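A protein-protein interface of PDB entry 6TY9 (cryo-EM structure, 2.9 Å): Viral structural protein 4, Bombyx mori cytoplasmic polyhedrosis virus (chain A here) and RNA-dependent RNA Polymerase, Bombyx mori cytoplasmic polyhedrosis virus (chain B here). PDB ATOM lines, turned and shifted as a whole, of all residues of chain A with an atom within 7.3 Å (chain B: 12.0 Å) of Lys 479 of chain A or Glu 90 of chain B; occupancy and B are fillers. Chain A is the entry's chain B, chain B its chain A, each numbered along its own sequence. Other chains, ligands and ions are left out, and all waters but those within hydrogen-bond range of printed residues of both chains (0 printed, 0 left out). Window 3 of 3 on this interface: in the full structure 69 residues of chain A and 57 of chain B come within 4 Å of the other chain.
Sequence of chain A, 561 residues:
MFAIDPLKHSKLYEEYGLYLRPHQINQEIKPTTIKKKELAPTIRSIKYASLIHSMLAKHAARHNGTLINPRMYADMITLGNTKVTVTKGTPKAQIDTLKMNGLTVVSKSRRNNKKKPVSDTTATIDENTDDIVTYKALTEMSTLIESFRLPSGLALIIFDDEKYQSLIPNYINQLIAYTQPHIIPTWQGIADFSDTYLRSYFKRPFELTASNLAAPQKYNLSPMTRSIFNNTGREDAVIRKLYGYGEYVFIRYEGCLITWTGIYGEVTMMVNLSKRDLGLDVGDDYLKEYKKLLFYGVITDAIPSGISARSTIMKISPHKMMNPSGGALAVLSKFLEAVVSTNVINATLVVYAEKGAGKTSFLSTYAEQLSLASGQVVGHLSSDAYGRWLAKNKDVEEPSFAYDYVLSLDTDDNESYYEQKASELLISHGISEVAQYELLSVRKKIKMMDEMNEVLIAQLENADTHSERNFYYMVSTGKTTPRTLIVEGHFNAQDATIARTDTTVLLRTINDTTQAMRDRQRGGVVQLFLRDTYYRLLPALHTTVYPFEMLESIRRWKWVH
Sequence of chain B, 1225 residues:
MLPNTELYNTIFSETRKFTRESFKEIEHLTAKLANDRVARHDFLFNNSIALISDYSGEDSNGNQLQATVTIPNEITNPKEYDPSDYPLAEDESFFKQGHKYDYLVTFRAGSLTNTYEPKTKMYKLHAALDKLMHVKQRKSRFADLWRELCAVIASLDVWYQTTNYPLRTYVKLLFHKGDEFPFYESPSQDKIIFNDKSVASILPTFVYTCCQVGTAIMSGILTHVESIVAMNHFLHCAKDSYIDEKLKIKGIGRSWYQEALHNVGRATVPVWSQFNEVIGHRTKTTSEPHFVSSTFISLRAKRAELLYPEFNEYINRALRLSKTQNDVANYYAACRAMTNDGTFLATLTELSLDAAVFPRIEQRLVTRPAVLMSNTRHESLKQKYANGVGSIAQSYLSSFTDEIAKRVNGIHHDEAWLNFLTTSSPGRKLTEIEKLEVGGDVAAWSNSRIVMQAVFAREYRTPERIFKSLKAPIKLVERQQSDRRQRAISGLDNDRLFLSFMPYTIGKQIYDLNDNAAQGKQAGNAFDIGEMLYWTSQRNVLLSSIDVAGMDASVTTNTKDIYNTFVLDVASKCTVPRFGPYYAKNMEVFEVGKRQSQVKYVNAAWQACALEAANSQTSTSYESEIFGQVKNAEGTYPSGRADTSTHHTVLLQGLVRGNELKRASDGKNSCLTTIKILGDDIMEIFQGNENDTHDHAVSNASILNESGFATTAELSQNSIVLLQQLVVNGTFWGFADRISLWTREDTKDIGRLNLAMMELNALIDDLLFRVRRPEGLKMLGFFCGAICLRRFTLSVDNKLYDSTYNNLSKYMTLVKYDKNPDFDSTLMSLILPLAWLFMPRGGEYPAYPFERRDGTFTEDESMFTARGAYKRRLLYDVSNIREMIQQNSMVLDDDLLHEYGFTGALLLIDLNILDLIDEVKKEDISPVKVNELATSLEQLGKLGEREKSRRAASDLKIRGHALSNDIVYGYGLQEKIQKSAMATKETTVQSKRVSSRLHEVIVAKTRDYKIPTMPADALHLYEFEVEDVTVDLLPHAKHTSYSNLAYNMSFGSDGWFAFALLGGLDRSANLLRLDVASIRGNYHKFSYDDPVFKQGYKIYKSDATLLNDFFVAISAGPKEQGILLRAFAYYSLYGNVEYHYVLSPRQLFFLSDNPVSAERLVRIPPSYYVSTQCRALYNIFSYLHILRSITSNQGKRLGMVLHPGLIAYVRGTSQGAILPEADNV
N of Ala 89 of chain B is in hydrogen-bond range of O of Phe 94 of chain B, 3.0 Å away. The backbone carbonyl oxygen (O) of Lys 96 of chain B is in hydrogen-bond range of a ring nitrogen (ND1) of His 99 of chain B (2.8 Å). The side-chain hydroxyl (OG) of Ser 476 of chain A is in hydrogen-bond range of the backbone carbonyl oxygen (O) of Tyr 473 of chain A, 3.5 Å away.
Of the 10 printed residues of chain A, 4 touch a printed residue of chain B. Printed residues of chain A that touch a printed residue of chain B: Tyr 473, Thr 477, Gly 478 and Lys 479. Printed residues of chain B that touch a printed residue of chain A: Ala 89, Glu 90, Asp 91, Ser 93, Lys 96 and Gln 97. Hydrophobic or aromatic side chains of chain B that line the printed part of chain A: Ala 89. Among the printed residues, 8 pairs touch across the chains. Among the printed residues, no Asp or Glu carboxylate lies within 4 Å of a Lys or Arg side-chain nitrogen of the other chain.
N of Asp 91 of chain B lies within hydrogen-bond range of O of Thr 477 of chain A (2.9 Å). OH of Tyr 473 of chain A is in hydrogen-bond range of N of Gln 97 of chain B, 3.1 Å away. The backbone carbonyl oxygen of Gly 478 of chain A sits close to the side-chain carboxylate of Asp 91 of chain B.
Among the printed residues, merely in contact across the chains: Lys 479 of chain A with Glu 90 of chain B, Tyr 473 of chain A with Lys 96 of chain B, Thr 477 of chain A with Glu 90 of chain B, Tyr 473 of chain A with Ala 89 of chain B and Thr 477 of chain A with Ser 93 of chain B.
Of chain B, only Glu 90, Asp 91 and Ser 93 come within 4 Å of Thr 477 of chain A. Of chain B, only Asp 91 comes within 4 Å of Gly 478 of chain A. Lys 479 of chain A touches one residue of chain B. No residue of chain B comes within 4 Å of Thr 480 of chain A. No residue of chain B comes within 4 Å of Thr 481 of chain A. Of the printed residues of chain A, Ala 89 of chain B touches Tyr 473. Glu 90 of chain B touches just these residues of chain A: Thr 477 (3.7 Å) and Lys 479 (3.2 Å). Printed residues of chain A within 4 Å of Asp 91 of chain B: Thr 477 (2.9 Å) and Gly 478 (3.4 Å). Of the printed residues of chain A, Ser 93 of chain B touches Thr 477. Of the printed residues of chain A, Lys 96 of chain B touches Tyr 473 (3.6 Å). Of the printed residues of chain A, Gln 97 of chain B touches Tyr 473. The nearest residue of chain B that does not touch Lys 479 of chain A is Asp 91 of chain B (4.3 Å). The nearest residue of chain A that does not touch Glu 90 of chain B is Gly 478 of chain A (5.0 Å). The nearest printed residue of chain A that does not touch Asp 91 of chain B is Ser 476 of chain A (4.1 Å).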
ATOM      1  N   TYR A 473      12.448  -0.686 -19.933  1.00  0.00           N
ATOM      2  CA  TYR A 473      12.472  -1.973 -20.616  1.00  0.00           C
ATOM      3  C   TYR A 473      11.062  -2.499 -20.829  1.00  0.00           C
ATOM      4  O   TYR A 473      10.707  -2.940 -21.926  1.00  0.00           O
ATOM      5  CB  TYR A 473      13.305  -2.968 -19.811  1.00  0.00           C
ATOM      6  CG  TYR A 473      13.106  -4.418 -20.186  1.00  0.00           C
ATOM      7  CD1 TYR A 473      13.729  -4.961 -21.297  1.00  0.00           C
ATOM      8  CD2 TYR A 473      12.309  -5.248 -19.417  1.00  0.00           C
ATOM      9  CE1 TYR A 473      13.556  -6.282 -21.635  1.00  0.00           C
ATOM     10  CE2 TYR A 473      12.130  -6.567 -19.749  1.00  0.00           C
ATOM     11  CZ  TYR A 473      12.756  -7.080 -20.857  1.00  0.00           C
ATOM     12  OH  TYR A 473      12.579  -8.399 -21.188  1.00  0.00           O
ATOM     13  N   MET A 474      10.236  -2.460 -19.785  1.00  0.00           N
ATOM     14  CA  MET A 474       8.880  -2.974 -19.905  1.00  0.00           C
ATOM     15  C   MET A 474       7.999  -2.081 -20.760  1.00  0.00           C
ATOM     16  O   MET A 474       6.958  -2.537 -21.237  1.00  0.00           O
ATOM     17  CB  MET A 474       8.262  -3.149 -18.520  1.00  0.00           C
ATOM     18  CG  MET A 474       8.974  -4.158 -17.641  1.00  0.00           C
ATOM     19  SD  MET A 474       8.872  -5.853 -18.233  1.00  0.00           S
ATOM     20  CE  MET A 474       7.120  -5.992 -18.546  1.00  0.00           C
ATOM     21  N   VAL A 475       8.382  -0.826 -20.962  1.00  0.00           N
ATOM     22  CA  VAL A 475       7.594   0.074 -21.794  1.00  0.00           C
ATOM     23  C   VAL A 475       7.978  -0.049 -23.259  1.00  0.00           C
ATOM     24  O   VAL A 475       7.110  -0.130 -24.126  1.00  0.00           O
ATOM     25  CB  VAL A 475       7.734   1.525 -21.296  1.00  0.00           C
ATOM     26  CG1 VAL A 475       7.043   2.472 -22.250  1.00  0.00           C
ATOM     27  CG2 VAL A 475       7.146   1.671 -19.917  1.00  0.00           C
ATOM     28  N   SER A 476       9.276  -0.079 -23.562  1.00  0.00           N
ATOM     29  CA  SER A 476       9.703  -0.147 -24.955  1.00  0.00           C
ATOM     30  C   SER A 476       9.410  -1.510 -25.564  1.00  0.00           C
ATOM     31  O   SER A 476       9.056  -1.604 -26.743  1.00  0.00           O
ATOM     32  CB  SER A 476      11.191   0.169 -25.065  1.00  0.00           C
ATOM     33  OG  SER A 476      11.939  -0.578 -24.127  1.00  0.00           O
ATOM     34  N   THR A 477       9.559  -2.577 -24.785  1.00  0.00           N
ATOM     35  CA  THR A 477       9.361  -3.939 -25.274  1.00  0.00           C
ATOM     36  C   THR A 477       7.923  -4.405 -25.101  1.00  0.00           C
ATOM     37  O   THR A 477       7.642  -5.601 -25.166  1.00  0.00           O
ATOM     38  CB  THR A 477      10.316  -4.901 -24.574  1.00  0.00           C
ATOM     39  OG1 THR A 477      10.160  -4.786 -23.157  1.00  0.00           O
ATOM     40  CG2 THR A 477      11.751  -4.592 -24.946  1.00  0.00           C
ATOM     41  N   GLY A 478       6.992  -3.486 -24.886  1.00  0.00           N
ATOM     42  CA  GLY A 478       5.603  -3.861 -24.759  1.00  0.00           C
ATOM     43  C   GLY A 478       4.974  -4.194 -26.091  1.00  0.00           C
ATOM     44  O   GLY A 478       5.455  -3.813 -27.154  1.00  0.00           O
ATOM     45  N   LYS A 479       3.862  -4.925 -26.021  1.00  0.00           N
ATOM     46  CA  LYS A 479       3.195  -5.390 -27.232  1.00  0.00           C
ATOM     47  C   LYS A 479       2.546  -4.237 -27.985  1.00  0.00           C
ATOM     48  O   LYS A 479       2.614  -4.166 -29.216  1.00  0.00           O
ATOM     49  CB  LYS A 479       2.153  -6.449 -26.872  1.00  0.00           C
ATOM     50  CG  LYS A 479       2.718  -7.834 -26.649  1.00  0.00           C
ATOM     51  CD  LYS A 479       2.676  -8.642 -27.924  1.00  0.00           C
ATOM     52  CE  LYS A 479       2.865 -10.116 -27.643  1.00  0.00           C
ATOM     53  NZ  LYS A 479       1.930 -10.603 -26.595  1.00  0.00           N
ATOM     54  N   THR A 480       1.908  -3.325 -27.263  1.00  0.00           N
ATOM     55  CA  THR A 480       1.155  -2.237 -27.867  1.00  0.00           C
ATOM     56  C   THR A 480       1.913  -0.917 -27.880  1.00  0.00           C
ATOM     57  O   THR A 480       1.314   0.124 -28.162  1.00  0.00           O
ATOM     58  CB  THR A 480      -0.177  -2.061 -27.140  1.00  0.00           C
ATOM     59  OG1 THR A 480       0.073  -1.765 -25.761  1.00  0.00           O
ATOM     60  CG2 THR A 480      -1.001  -3.324 -27.234  1.00  0.00           C
ATOM     61  N   THR A 481       3.207  -0.934 -27.580  1.00  0.00           N
ATOM     62  CA  THR A 481       3.998   0.282 -27.618  1.00  0.00           C
ATOM     63  C   THR A 481       4.398   0.595 -29.058  1.00  0.00           C
ATOM     64  O   THR A 481       4.732  -0.311 -29.824  1.00  0.00           O
ATOM     65  CB  THR A 481       5.244   0.122 -26.754  1.00  0.00           C
ATOM     66  OG1 THR A 481       4.856  -0.211 -25.418  1.00  0.00           O
ATOM     67  CG2 THR A 481       6.048   1.401 -26.720  1.00  0.00           C
ATOM     68  N   PRO A 482       4.356   1.865 -29.456  1.00  0.00           N
ATOM     69  CA  PRO A 482       4.773   2.223 -30.813  1.00  0.00           C
ATOM     70  C   PRO A 482       6.175   1.734 -31.130  1.00  0.00           C
ATOM     71  O   PRO A 482       7.024   1.556 -30.257  1.00  0.00           O
ATOM     72  CB  PRO A 482       4.705   3.749 -30.805  1.00  0.00           C
ATOM     73  CG  PRO A 482       3.660   4.052 -29.832  1.00  0.00           C
ATOM     74  CD  PRO A 482       3.763   3.016 -28.757  1.00  0.00           C
ATOM     75  N   PRO B  83      11.534 -25.206 -23.710  1.00  0.00           N
ATOM     76  CA  PRO B  83      11.642 -23.921 -24.415  1.00  0.00           C
ATOM     77  C   PRO B  83      11.585 -22.709 -23.502  1.00  0.00           C
ATOM     78  O   PRO B  83      11.846 -21.597 -23.971  1.00  0.00           O
ATOM     79  CB  PRO B  83      10.450 -23.948 -25.376  1.00  0.00           C
ATOM     80  CG  PRO B  83       9.497 -24.898 -24.766  1.00  0.00           C
ATOM     81  CD  PRO B  83      10.310 -25.936 -24.075  1.00  0.00           C
ATOM     82  N   SER B  84      11.262 -22.880 -22.228  1.00  0.00           N
ATOM     83  CA  SER B  84      11.243 -21.778 -21.281  1.00  0.00           C
ATOM     84  C   SER B  84      12.613 -21.483 -20.693  1.00  0.00           C
ATOM     85  O   SER B  84      12.728 -20.599 -19.839  1.00  0.00           O
ATOM     86  CB  SER B  84      10.263 -22.072 -20.149  1.00  0.00           C
ATOM     87  OG  SER B  84      10.908 -22.800 -19.121  1.00  0.00           O
ATOM     88  N   TYR B  86      15.050 -20.388 -22.515  1.00  0.00           N
ATOM     89  CA  TYR B  86      15.533 -19.270 -23.319  1.00  0.00           C
ATOM     90  C   TYR B  86      14.341 -18.391 -23.672  1.00  0.00           C
ATOM     91  O   TYR B  86      13.852 -18.424 -24.810  1.00  0.00           O
ATOM     92  CB  TYR B  86      16.243 -19.754 -24.578  1.00  0.00           C
ATOM     93  CG  TYR B  86      17.416 -20.660 -24.311  1.00  0.00           C
ATOM     94  CD1 TYR B  86      18.630 -20.148 -23.891  1.00  0.00           C
ATOM     95  CD2 TYR B  86      17.311 -22.027 -24.488  1.00  0.00           C
ATOM     96  CE1 TYR B  86      19.703 -20.971 -23.650  1.00  0.00           C
ATOM     97  CE2 TYR B  86      18.379 -22.858 -24.252  1.00  0.00           C
ATOM     98  CZ  TYR B  86      19.572 -22.325 -23.833  1.00  0.00           C
ATOM     99  OH  TYR B  86      20.640 -23.152 -23.599  1.00  0.00           O
ATOM    100  N   PRO B  87      13.847 -17.597 -22.729  1.00  0.00           N
ATOM    101  CA  PRO B  87      12.648 -16.799 -22.997  1.00  0.00           C
ATOM    102  C   PRO B  87      12.924 -15.601 -23.888  1.00  0.00           C
ATOM    103  O   PRO B  87      14.072 -15.337 -24.251  1.00  0.00           O
ATOM    104  CB  PRO B  87      12.205 -16.366 -21.597  1.00  0.00           C
ATOM    105  CG  PRO B  87      13.451 -16.339 -20.809  1.00  0.00           C
ATOM    106  CD  PRO B  87      14.326 -17.426 -21.347  1.00  0.00           C
ATOM    107  N   LEU B  88      11.873 -14.870 -24.248  1.00  0.00           N
ATOM    108  CA  LEU B  88      12.004 -13.653 -25.033  1.00  0.00           C
ATOM    109  C   LEU B  88      11.169 -12.559 -24.387  1.00  0.00           C
ATOM    110  O   LEU B  88      10.334 -12.818 -23.519  1.00  0.00           O
ATOM    111  CB  LEU B  88      11.563 -13.860 -26.485  1.00  0.00           C
ATOM    112  CG  LEU B  88      12.288 -14.921 -27.309  1.00  0.00           C
ATOM    113  CD1 LEU B  88      11.634 -15.081 -28.660  1.00  0.00           C
ATOM    114  CD2 LEU B  88      13.744 -14.561 -27.472  1.00  0.00           C
ATOM    115  N   ALA B  89      11.405 -11.327 -24.821  1.00  0.00           N
ATOM    116  CA  ALA B  89      10.602 -10.207 -24.368  1.00  0.00           C
ATOM    117  C   ALA B  89       9.218 -10.258 -25.011  1.00  0.00           C
ATOM    118  O   ALA B  89       9.007 -10.899 -26.041  1.00  0.00           O
ATOM    119  CB  ALA B  89      11.296  -8.889 -24.689  1.00  0.00           C
ATOM    120  N   GLU B  90       8.259  -9.574 -24.385  1.00  0.00           N
ATOM    121  CA  GLU B  90       6.896  -9.582 -24.903  1.00  0.00           C
ATOM    122  C   GLU B  90       6.823  -9.058 -26.330  1.00  0.00           C
ATOM    123  O   GLU B  90       5.977  -9.508 -27.107  1.00  0.00           O
ATOM    124  CB  GLU B  90       5.988  -8.763 -23.993  1.00  0.00           C
ATOM    125  CG  GLU B  90       6.134  -9.106 -22.528  1.00  0.00           C
ATOM    126  CD  GLU B  90       5.933 -10.582 -22.250  1.00  0.00           C
ATOM    127  OE1 GLU B  90       4.836 -11.101 -22.549  1.00  0.00           O
ATOM    128  OE2 GLU B  90       6.868 -11.226 -21.729  1.00  0.00           O
ATOM    129  N   ASP B  91       7.694  -8.119 -26.693  1.00  0.00           N
ATOM    130  CA  ASP B  91       7.809  -7.701 -28.082  1.00  0.00           C
ATOM    131  C   ASP B  91       8.589  -8.699 -28.926  1.00  0.00           C
ATOM    132  O   ASP B  91       8.558  -8.598 -30.156  1.00  0.00           O
ATOM    133  CB  ASP B  91       8.476  -6.328 -28.154  1.00  0.00           C
ATOM    134  CG  ASP B  91       7.881  -5.451 -29.229  1.00  0.00           C
ATOM    135  OD1 ASP B  91       6.760  -5.756 -29.684  1.00  0.00           O
ATOM    136  OD2 ASP B  91       8.528  -4.455 -29.618  1.00  0.00           O
ATOM    137  N   GLU B  92       9.284  -9.648 -28.292  1.00  0.00           N
ATOM    138  CA  GLU B  92      10.124 -10.634 -28.975  1.00  0.00           C
ATOM    139  C   GLU B  92      11.237  -9.965 -29.772  1.00  0.00           C
ATOM    140  O   GLU B  92      11.728 -10.500 -30.765  1.00  0.00           O
ATOM    141  CB  GLU B  92       9.291 -11.548 -29.869  1.00  0.00           C
ATOM    142  CG  GLU B  92       8.488 -12.577 -29.112  1.00  0.00           C
ATOM    143  CD  GLU B  92       7.874 -13.603 -30.027  1.00  0.00           C
ATOM    144  OE1 GLU B  92       7.950 -13.416 -31.257  1.00  0.00           O
ATOM    145  OE2 GLU B  92       7.316 -14.596 -29.520  1.00  0.00           O
ATOM    146  N   SER B  93      11.648  -8.783 -29.323  1.00  0.00           N
ATOM    147  CA  SER B  93      12.737  -8.062 -29.960  1.00  0.00           C
ATOM    148  C   SER B  93      14.105  -8.486 -29.456  1.00  0.00           C
ATOM    149  O   SER B  93      15.104  -8.227 -30.133  1.00  0.00           O
ATOM    150  CB  SER B  93      12.569  -6.558 -29.744  1.00  0.00           C
ATOM    151  OG  SER B  93      12.471  -6.270 -28.365  1.00  0.00           O
ATOM    152  N   PHE B  94      14.170  -9.126 -28.294  1.00  0.00           N
ATOM    153  CA  PHE B  94      15.418  -9.632 -27.748  1.00  0.00           C
ATOM    154  C   PHE B  94      15.078 -10.643 -26.665  1.00  0.00           C
ATOM    155  O   PHE B  94      13.914 -10.822 -26.303  1.00  0.00           O
ATOM    156  CB  PHE B  94      16.288  -8.500 -27.198  1.00  0.00           C
ATOM    157  CG  PHE B  94      17.720  -8.883 -26.995  1.00  0.00           C
ATOM    158  CD1 PHE B  94      18.512  -9.233 -28.068  1.00  0.00           C
ATOM    159  CD2 PHE B  94      18.270  -8.901 -25.733  1.00  0.00           C
ATOM    160  CE1 PHE B  94      19.822  -9.591 -27.884  1.00  0.00           C
ATOM    161  CE2 PHE B  94      19.580  -9.257 -25.545  1.00  0.00           C
ATOM    162  CZ  PHE B  94      20.356  -9.603 -26.623  1.00  0.00           C
ATOM    163  N   PHE B  95      16.108 -11.309 -26.159  1.00  0.00           N
ATOM    164  CA  PHE B  95      15.941 -12.202 -25.027  1.00  0.00           C
ATOM    165  C   PHE B  95      15.427 -11.435 -23.814  1.00  0.00           C
ATOM    166  O   PHE B  95      15.577 -10.217 -23.708  1.00  0.00           O
ATOM    167  CB  PHE B  95      17.261 -12.887 -24.689  1.00  0.00           C
ATOM    168  CG  PHE B  95      17.623 -13.991 -25.629  1.00  0.00           C
ATOM    169  CD1 PHE B  95      16.901 -15.169 -25.639  1.00  0.00           C
ATOM    170  CD2 PHE B  95      18.684 -13.857 -26.501  1.00  0.00           C
ATOM    171  CE1 PHE B  95      17.228 -16.186 -26.503  1.00  0.00           C
ATOM    172  CE2 PHE B  95      19.016 -14.878 -27.366  1.00  0.00           C
ATOM    173  CZ  PHE B  95      18.287 -16.042 -27.367  1.00  0.00           C
ATOM    174  N   LYS B  96      14.812 -12.166 -22.892  1.00  0.00           N
ATOM    175  CA  LYS B  96      14.292 -11.565 -21.674  1.00  0.00           C
ATOM    176  C   LYS B  96      15.407 -10.860 -20.909  1.00  0.00           C
ATOM    177  O   LYS B  96      16.589 -11.168 -21.067  1.00  0.00           O
ATOM    178  CB  LYS B  96      13.637 -12.627 -20.797  1.00  0.00           C
ATOM    179  CG  LYS B  96      12.659 -12.071 -19.796  1.00  0.00           C
ATOM    180  CD  LYS B  96      12.007 -13.162 -18.981  1.00  0.00           C
ATOM    181  CE  LYS B  96      10.985 -12.573 -18.034  1.00  0.00           C
ATOM    182  NZ  LYS B  96      10.199 -13.615 -17.332  1.00  0.00           N
ATOM    183  N   GLN B  97      15.020  -9.895 -20.077  1.00  0.00           N
ATOM    184  CA  GLN B  97      15.997  -9.052 -19.399  1.00  0.00           C
ATOM    185  C   GLN B  97      16.893  -9.867 -18.480  1.00  0.00           C
ATOM    186  O   GLN B  97      18.095  -9.995 -18.734  1.00  0.00           O
ATOM    187  CB  GLN B  97      15.293  -7.956 -18.606  1.00  0.00           C
ATOM    188  CG  GLN B  97      16.163  -6.760 -18.295  1.00  0.00           C
ATOM    189  CD  GLN B  97      15.487  -5.782 -17.365  1.00  0.00           C
ATOM    190  OE1 GLN B  97      14.565  -6.135 -16.634  1.00  0.00           O
ATOM    191  NE2 GLN B  97      15.936  -4.540 -17.393  1.00  0.00           N
ATOM    192  N   GLY B  98      16.331 -10.422 -17.415  1.00  0.00           N
ATOM    193  CA  GLY B  98      17.112 -11.303 -16.574  1.00  0.00           C
ATOM    194  C   GLY B  98      16.810 -12.753 -16.865  1.00  0.00           C
ATOM    195  O   GLY B  98      15.818 -13.291 -16.367  1.00  0.00           O
ATOM    196  N   HIS B  99      17.652 -13.407 -17.655  1.00  0.00           N
ATOM    197  CA  HIS B  99      17.440 -14.794 -18.024  1.00  0.00           C
ATOM    198  C   HIS B  99      18.544 -15.646 -17.420  1.00  0.00           C
ATOM    199  O   HIS B  99      19.702 -15.225 -17.358  1.00  0.00           O
ATOM    200  CB  HIS B  99      17.373 -14.961 -19.545  1.00  0.00           C
ATOM    201  CG  HIS B  99      18.559 -14.418 -20.277  1.00  0.00           C
ATOM    202  ND1 HIS B  99      18.502 -13.270 -21.033  1.00  0.00           N
ATOM    203  CD2 HIS B  99      19.824 -14.881 -20.394  1.00  0.00           C
ATOM    204  CE1 HIS B  99      19.685 -13.039 -21.573  1.00  0.00           C
ATOM    205  NE2 HIS B  99      20.505 -14.005 -21.202  1.00  0.00           N
ATOM    206  N   LYS B 121       9.873 -15.928 -36.222  1.00  0.00           N
ATOM    207  CA  LYS B 121      10.703 -15.668 -35.051  1.00  0.00           C
ATOM    208  C   LYS B 121      11.087 -16.958 -34.336  1.00  0.00           C
ATOM    209  O   LYS B 121      12.270 -17.191 -34.071  1.00  0.00           O
ATOM    210  CB  LYS B 121       9.982 -14.714 -34.101  1.00  0.00           C
ATOM    211  CG  LYS B 121      10.830 -14.218 -32.946  1.00  0.00           C
ATOM    212  CD  LYS B 121      12.168 -13.679 -33.419  1.00  0.00           C
ATOM    213  CE  LYS B 121      12.017 -12.418 -34.238  1.00  0.00           C
ATOM    214  NZ  LYS B 121      11.368 -11.339 -33.462  1.00  0.00           N
ATOM    215  N   MET B 122      10.112 -17.814 -34.025  1.00  0.00           N
ATOM    216  CA  MET B 122      10.427 -19.041 -33.300  1.00  0.00           C
ATOM    217  C   MET B 122      11.212 -20.022 -34.159  1.00  0.00           C
ATOM    218  O   MET B 122      11.906 -20.892 -33.626  1.00  0.00           O
ATOM    219  CB  MET B 122       9.150 -19.691 -32.782  1.00  0.00           C
ATOM    220  CG  MET B 122       8.424 -18.878 -31.731  1.00  0.00           C
ATOM    221  SD  MET B 122       9.447 -18.468 -30.308  1.00  0.00           S
ATOM    222  CE  MET B 122      10.022 -20.087 -29.818  1.00  0.00           C
ATOM    223  N   LEU B 125      14.805 -18.618 -33.721  1.00  0.00           N
ATOM    224  CA  LEU B 125      15.318 -18.932 -32.393  1.00  0.00           C
ATOM    225  C   LEU B 125      15.778 -20.378 -32.308  1.00  0.00           C
ATOM    226  O   LEU B 125      16.732 -20.688 -31.589  1.00  0.00           O
ATOM    227  CB  LEU B 125      14.254 -18.643 -31.339  1.00  0.00           C
ATOM    228  CG  LEU B 125      14.631 -18.911 -29.883  1.00  0.00           C
ATOM    229  CD1 LEU B 125      14.134 -17.796 -29.010  1.00  0.00           C
ATOM    230  CD2 LEU B 125      14.035 -20.215 -29.420  1.00  0.00           C
ATOM    231  N   PHE B 627      17.101 -11.592 -34.313  1.00  0.00           N
ATOM    232  CA  PHE B 627      16.413 -10.337 -34.039  1.00  0.00           C
ATOM    233  C   PHE B 627      16.770  -9.213 -34.998  1.00  0.00           C
ATOM    234  O   PHE B 627      16.240  -8.110 -34.846  1.00  0.00           O
ATOM    235  CB  PHE B 627      16.711  -9.875 -32.612  1.00  0.00           C
ATOM    236  CG  PHE B 627      16.458 -10.922 -31.575  1.00  0.00           C
ATOM    237  CD1 PHE B 627      15.171 -11.276 -31.235  1.00  0.00           C
ATOM    238  CD2 PHE B 627      17.509 -11.548 -30.939  1.00  0.00           C
ATOM    239  CE1 PHE B 627      14.940 -12.233 -30.284  1.00  0.00           C
ATOM    240  CE2 PHE B 627      17.277 -12.505 -29.983  1.00  0.00           C
ATOM    241  CZ  PHE B 627      15.993 -12.847 -29.659  1.00  0.00           C
